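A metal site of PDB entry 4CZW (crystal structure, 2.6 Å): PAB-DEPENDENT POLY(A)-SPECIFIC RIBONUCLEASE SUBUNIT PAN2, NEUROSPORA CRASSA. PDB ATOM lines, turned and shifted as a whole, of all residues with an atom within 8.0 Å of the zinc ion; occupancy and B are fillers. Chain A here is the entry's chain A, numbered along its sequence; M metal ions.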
ATOM      1  N   LYS A 189      16.588  -0.181  11.290  1.00  0.00           N
ATOM      2  CA  LYS A 189      15.380  -0.605  10.592  1.00  0.00           C
ATOM      3  C   LYS A 189      15.693  -1.258   9.252  1.00  0.00           C
ATOM      4  O   LYS A 189      16.393  -0.679   8.417  1.00  0.00           O
ATOM      5  CB  LYS A 189      14.441   0.586  10.387  1.00  0.00           C
ATOM      6  CG  LYS A 189      13.209   0.257   9.550  1.00  0.00           C
ATOM      7  CD  LYS A 189      12.385   1.508   9.269  1.00  0.00           C
ATOM      8  CE  LYS A 189      11.819   2.102  10.535  1.00  0.00           C
ATOM      9  NZ  LYS A 189      10.957   3.287  10.265  1.00  0.00           N
ATOM     10  N   CYS A 190      15.170  -2.462   9.050  1.00  0.00           N
ATOM     11  CA  CYS A 190      15.249  -3.124   7.754  1.00  0.00           C
ATOM     12  C   CYS A 190      14.399  -2.351   6.753  1.00  0.00           C
ATOM     13  O   CYS A 190      13.230  -2.074   7.007  1.00  0.00           O
ATOM     14  CB  CYS A 190      14.788  -4.573   7.844  1.00  0.00           C
ATOM     15  SG  CYS A 190      14.690  -5.449   6.260  1.00  0.00           S
ATOM     16  N   MET A 191      14.987  -2.015   5.606  1.00  0.00           N
ATOM     17  CA  MET A 191      14.280  -1.204   4.616  1.00  0.00           C
ATOM     18  C   MET A 191      13.359  -2.042   3.730  1.00  0.00           C
ATOM     19  O   MET A 191      12.791  -1.537   2.762  1.00  0.00           O
ATOM     20  CB  MET A 191      15.269  -0.433   3.748  1.00  0.00           C
ATOM     21  CG  MET A 191      16.110   0.577   4.536  1.00  0.00           C
ATOM     22  SD  MET A 191      17.241   1.663   3.384  1.00  0.00           S
ATOM     23  CE  MET A 191      15.853   2.531   2.330  1.00  0.00           C
ATOM     24  N   HIS A 192      13.208  -3.323   4.061  1.00  0.00           N
ATOM     25  CA  HIS A 192      12.331  -4.207   3.302  1.00  0.00           C
ATOM     26  C   HIS A 192      11.056  -4.533   4.075  1.00  0.00           C
ATOM     27  O   HIS A 192       9.950  -4.232   3.634  1.00  0.00           O
ATOM     28  CB  HIS A 192      13.062  -5.494   2.919  1.00  0.00           C
ATOM     29  CG  HIS A 192      12.295  -6.349   1.952  1.00  0.00           C
ATOM     30  ND1 HIS A 192      12.092  -5.993   0.642  1.00  0.00           N
ATOM     31  CD2 HIS A 192      11.685  -7.548   2.116  1.00  0.00           C
ATOM     32  CE1 HIS A 192      11.396  -6.937   0.031  1.00  0.00           C
ATOM     33  NE2 HIS A 192      11.136  -7.889   0.904  1.00  0.00           N
ATOM     34  N   CYS A 193      11.213  -5.154   5.244  1.00  0.00           N
ATOM     35  CA  CYS A 193      10.074  -5.564   6.053  1.00  0.00           C
ATOM     36  C   CYS A 193       9.801  -4.577   7.191  1.00  0.00           C
ATOM     37  O   CYS A 193       8.963  -4.833   8.056  1.00  0.00           O
ATOM     38  CB  CYS A 193      10.292  -6.969   6.622  1.00  0.00           C
ATOM     39  SG  CYS A 193      11.685  -7.104   7.765  1.00  0.00           S
ATOM     40  N   GLN A 194      10.532  -3.469   7.193  1.00  0.00           N
ATOM     41  CA  GLN A 194      10.347  -2.381   8.153  1.00  0.00           C
ATOM     42  C   GLN A 194      10.497  -2.820   9.604  1.00  0.00           C
ATOM     43  O   GLN A 194       9.946  -2.189  10.508  1.00  0.00           O
ATOM     44  CB  GLN A 194       8.971  -1.732   7.942  1.00  0.00           C
ATOM     45  CG  GLN A 194       8.672  -1.382   6.491  1.00  0.00           C
ATOM     46  CD  GLN A 194       9.767  -0.553   5.846  1.00  0.00           C
ATOM     47  OE1 GLN A 194      10.269   0.401   6.441  1.00  0.00           O
ATOM     48  NE2 GLN A 194      10.147  -0.921   4.626  1.00  0.00           N
ATOM     49  N   HIS A 195      11.247  -3.893   9.831  1.00  0.00           N
ATOM     50  CA  HIS A 195      11.494  -4.379  11.181  1.00  0.00           C
ATOM     51  C   HIS A 195      12.584  -3.561  11.871  1.00  0.00           C
ATOM     52  O   HIS A 195      13.603  -3.241  11.265  1.00  0.00           O
ATOM     53  CB  HIS A 195      11.893  -5.857  11.156  1.00  0.00           C
ATOM     54  CG  HIS A 195      12.193  -6.433  12.514  1.00  0.00           C
ATOM     55  ND1 HIS A 195      11.249  -6.521  13.505  1.00  0.00           N
ATOM     56  CD2 HIS A 195      13.337  -6.929  13.034  1.00  0.00           C
ATOM     57  CE1 HIS A 195      11.788  -7.060  14.580  1.00  0.00           C
ATOM     58  NE2 HIS A 195      13.058  -7.321  14.317  1.00  0.00           N
ATOM     59  N   VAL A 196      12.356  -3.220  13.137  1.00  0.00           N
ATOM     60  CA  VAL A 196      13.302  -2.406  13.890  1.00  0.00           C
ATOM     61  C   VAL A 196      13.965  -3.181  15.024  1.00  0.00           C
ATOM     62  O   VAL A 196      13.322  -3.989  15.697  1.00  0.00           O
ATOM     63  CB  VAL A 196      12.625  -1.143  14.473  1.00  0.00           C
ATOM     64  CG1 VAL A 196      12.303  -0.157  13.361  1.00  0.00           C
ATOM     65  CG2 VAL A 196      11.371  -1.522  15.239  1.00  0.00           C
ATOM     66  N   GLY A 243      23.081  -5.369   5.900  1.00  0.00           N
ATOM     67  CA  GLY A 243      23.185  -6.254   7.050  1.00  0.00           C
ATOM     68  C   GLY A 243      22.067  -7.265   7.066  1.00  0.00           C
ATOM     69  O   GLY A 243      21.058  -7.101   6.374  1.00  0.00           O
ATOM     70  N   TYR A 244      22.244  -8.316   7.858  1.00  0.00           N
ATOM     71  CA  TYR A 244      21.258  -9.390   7.920  1.00  0.00           C
ATOM     72  C   TYR A 244      20.018  -8.971   8.701  1.00  0.00           C
ATOM     73  O   TYR A 244      20.108  -8.239   9.680  1.00  0.00           O
ATOM     74  CB  TYR A 244      21.872 -10.637   8.558  1.00  0.00           C
ATOM     75  CG  TYR A 244      21.025 -11.888   8.404  1.00  0.00           C
ATOM     76  CD1 TYR A 244      21.098 -12.662   7.263  1.00  0.00           C
ATOM     77  CD2 TYR A 244      20.162 -12.284   9.423  1.00  0.00           C
ATOM     78  CE1 TYR A 244      20.331 -13.804   7.118  1.00  0.00           C
ATOM     79  CE2 TYR A 244      19.390 -13.425   9.286  1.00  0.00           C
ATOM     80  CZ  TYR A 244      19.478 -14.180   8.131  1.00  0.00           C
ATOM     81  OH  TYR A 244      18.714 -15.312   7.987  1.00  0.00           O
ATOM     82  N   CYS A 245      18.855  -9.421   8.246  1.00  0.00           N
ATOM     83  CA  CYS A 245      17.610  -9.178   8.954  1.00  0.00           C
ATOM     84  C   CYS A 245      16.992 -10.499   9.399  1.00  0.00           C
ATOM     85  O   CYS A 245      16.733 -11.380   8.573  1.00  0.00           O
ATOM     86  CB  CYS A 245      16.619  -8.395   8.096  1.00  0.00           C
ATOM     87  SG  CYS A 245      15.050  -8.052   8.924  1.00  0.00           S
ATOM     88  N   THR A 246      16.759 -10.626  10.695  1.00  0.00           N
ATOM     89  CA  THR A 246      16.251 -11.872  11.264  1.00  0.00           C
ATOM     90  C   THR A 246      14.817 -12.171  10.828  1.00  0.00           C
ATOM     91  O   THR A 246      14.406 -13.335  10.804  1.00  0.00           O
ATOM     92  CB  THR A 246      16.311 -11.848  12.802  1.00  0.00           C
ATOM     93  OG1 THR A 246      15.568 -10.731  13.299  1.00  0.00           O
ATOM     94  CG2 THR A 246      17.750 -11.745  13.277  1.00  0.00           C
ATOM     95  N   LYS A 247      14.064 -11.140  10.498  1.00  0.00           N
ATOM     96  CA  LYS A 247      12.656 -11.318  10.142  1.00  0.00           C
ATOM     97  C   LYS A 247      12.509 -11.917   8.738  1.00  0.00           C
ATOM     98  O   LYS A 247      11.937 -12.995   8.580  1.00  0.00           O
ATOM     99  CB  LYS A 247      11.897  -9.994  10.231  1.00  0.00           C
ATOM    100  CG  LYS A 247      10.382 -10.155  10.122  1.00  0.00           C
ATOM    101  CD  LYS A 247       9.664  -8.831  10.258  1.00  0.00           C
ATOM    102  CE  LYS A 247       8.154  -9.012  10.154  1.00  0.00           C
ATOM    103  NZ  LYS A 247       7.422  -7.720  10.202  1.00  0.00           N
ATOM    104  N   CYS A 248      13.012 -11.214   7.726  1.00  0.00           N
ATOM    105  CA  CYS A 248      12.892 -11.698   6.352  1.00  0.00           C
ATOM    106  C   CYS A 248      14.058 -12.603   5.968  1.00  0.00           C
ATOM    107  O   CYS A 248      14.249 -12.926   4.799  1.00  0.00           O
ATOM    108  CB  CYS A 248      12.777 -10.520   5.373  1.00  0.00           C
ATOM    109  SG  CYS A 248      13.982  -9.187   5.606  1.00  0.00           S
ATOM    110  N   GLN A 249      14.846 -13.001   6.967  1.00  0.00           N
ATOM    111  CA  GLN A 249      15.844 -14.063   6.828  1.00  0.00           C
ATOM    112  C   GLN A 249      16.880 -13.848   5.726  1.00  0.00           C
ATOM    113  O   GLN A 249      17.345 -14.815   5.128  1.00  0.00           O
ATOM    114  CB  GLN A 249      15.134 -15.399   6.596  1.00  0.00           C
ATOM    115  CG  GLN A 249      14.396 -15.940   7.810  1.00  0.00           C
ATOM    116  CD  GLN A 249      15.329 -16.623   8.797  1.00  0.00           C
ATOM    117  OE1 GLN A 249      15.610 -16.090   9.875  1.00  0.00           O
ATOM    118  NE2 GLN A 249      15.818 -17.804   8.433  1.00  0.00           N
ATOM    119  N   ARG A 250      17.245 -12.596   5.478  1.00  0.00           N
ATOM    120  CA  ARG A 250      18.259 -12.304   4.471  1.00  0.00           C
ATOM    121  C   ARG A 250      18.910 -10.947   4.668  1.00  0.00           C
ATOM    122  O   ARG A 250      18.430 -10.123   5.440  1.00  0.00           O
ATOM    123  CB  ARG A 250      17.652 -12.388   3.060  1.00  0.00           C
ATOM    124  CG  ARG A 250      16.520 -11.408   2.812  1.00  0.00           C
ATOM    125  CD  ARG A 250      16.040 -11.488   1.375  1.00  0.00           C
ATOM    126  NE  ARG A 250      17.113 -11.180   0.427  1.00  0.00           N
ATOM    127  CZ  ARG A 250      16.986 -11.241  -0.893  1.00  0.00           C
ATOM    128  NH1 ARG A 250      15.822 -11.583  -1.431  1.00  0.00           N
ATOM    129  NH2 ARG A 250      18.013 -10.939  -1.672  1.00  0.00           N
ATOM    130  N   TYR A 251      20.020 -10.723   3.959  1.00  0.00           N
ATOM    131  CA  TYR A 251      20.753  -9.460   4.046  1.00  0.00           C
ATOM    132  C   TYR A 251      20.033  -8.360   3.276  1.00  0.00           C
ATOM    133  O   TYR A 251      19.766  -8.490   2.078  1.00  0.00           O
ATOM    134  CB  TYR A 251      22.178  -9.643   3.518  1.00  0.00           C
ATOM    135  CG  TYR A 251      23.014 -10.583   4.348  1.00  0.00           C
ATOM    136  CD1 TYR A 251      22.974 -11.958   4.118  1.00  0.00           C
ATOM    137  CD2 TYR A 251      23.840 -10.105   5.353  1.00  0.00           C
ATOM    138  CE1 TYR A 251      23.741 -12.822   4.877  1.00  0.00           C
ATOM    139  CE2 TYR A 251      24.614 -10.970   6.118  1.00  0.00           C
ATOM    140  CZ  TYR A 251      24.553 -12.331   5.870  1.00  0.00           C
ATOM    141  OH  TYR A 251      25.320 -13.194   6.628  1.00  0.00           O
ATOM    142  N   GLN A 252      19.725  -7.272   3.971  1.00  0.00           N
ATOM    143  CA  GLN A 252      19.028  -6.138   3.373  1.00  0.00           C
ATOM    144  C   GLN A 252      19.739  -4.837   3.659  1.00  0.00           C
ATOM    145  O   GLN A 252      20.693  -4.797   4.440  1.00  0.00           O
ATOM    146  CB  GLN A 252      17.581  -6.064   3.900  1.00  0.00           C
ATOM    147  CG  GLN A 252      16.801  -7.361   3.828  1.00  0.00           C
ATOM    148  CD  GLN A 252      16.202  -7.622   2.458  1.00  0.00           C
ATOM    149  OE1 GLN A 252      16.734  -7.176   1.440  1.00  0.00           O
ATOM    150  NE2 GLN A 252      15.079  -8.334   2.431  1.00  0.00           N
ATOM    151  N   ASN A 253      19.295  -3.756   3.010  1.00  0.00           N
ATOM    152  CA  ASN A 253      19.745  -2.422   3.368  1.00  0.00           C
ATOM    153  C   ASN A 253      19.124  -2.016   4.700  1.00  0.00           C
ATOM    154  O   ASN A 253      17.914  -2.072   4.871  1.00  0.00           O
ATOM    155  CB  ASN A 253      19.386  -1.411   2.276  1.00  0.00           C
ATOM    156  CG  ASN A 253      20.246  -1.565   1.036  1.00  0.00           C
ATOM    157  OD1 ASN A 253      21.419  -1.919   1.109  1.00  0.00           O
ATOM    158  ND2 ASN A 253      19.654  -1.285  -0.122  1.00  0.00           N
ATOM    159  N   LEU A 254      19.970  -1.608   5.647  1.00  0.00           N
ATOM    160  CA  LEU A 254      19.491  -1.265   6.981  1.00  0.00           C
ATOM    161  C   LEU A 254      19.588   0.231   7.252  1.00  0.00           C
ATOM    162  O   LEU A 254      20.657   0.820   7.138  1.00  0.00           O
ATOM    163  CB  LEU A 254      20.266  -2.051   8.038  1.00  0.00           C
ATOM    164  CG  LEU A 254      20.260  -3.571   7.906  1.00  0.00           C
ATOM    165  CD1 LEU A 254      20.946  -4.222   9.091  1.00  0.00           C
ATOM    166  CD2 LEU A 254      18.844  -4.107   7.738  1.00  0.00           C
HETATM  167 ZN    ZN M   1      13.808  -7.432   7.112  1.00  0.00          ZN
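N of His 192 sits close to SG of Cys 190.
N of Cys 190 is in hydrogen-bond range of O of His 195 (2.8 Å).
The side-chain amide nitrogen (NE2) of Gln 252 lies close to the side-chain sulfur (SG) of Cys 248.
The backbone NH (N) of Lys 247 sits close to the side-chain sulfur (SG) of Cys 245.
The backbone NH of Cys 245 lies within hydrogen-bond range of the backbone carbonyl oxygen of Arg 250, 2.9 Å away.
The zinc ion is bound by the side-chain sulfur of Cys 193 (2.2 Å), the side-chain sulfur of Cys 245 (2.3 Å), the side-chain sulfur of Cys 248 (2.3 Å) and the side-chain sulfur of Cys 190 (2.3 Å).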
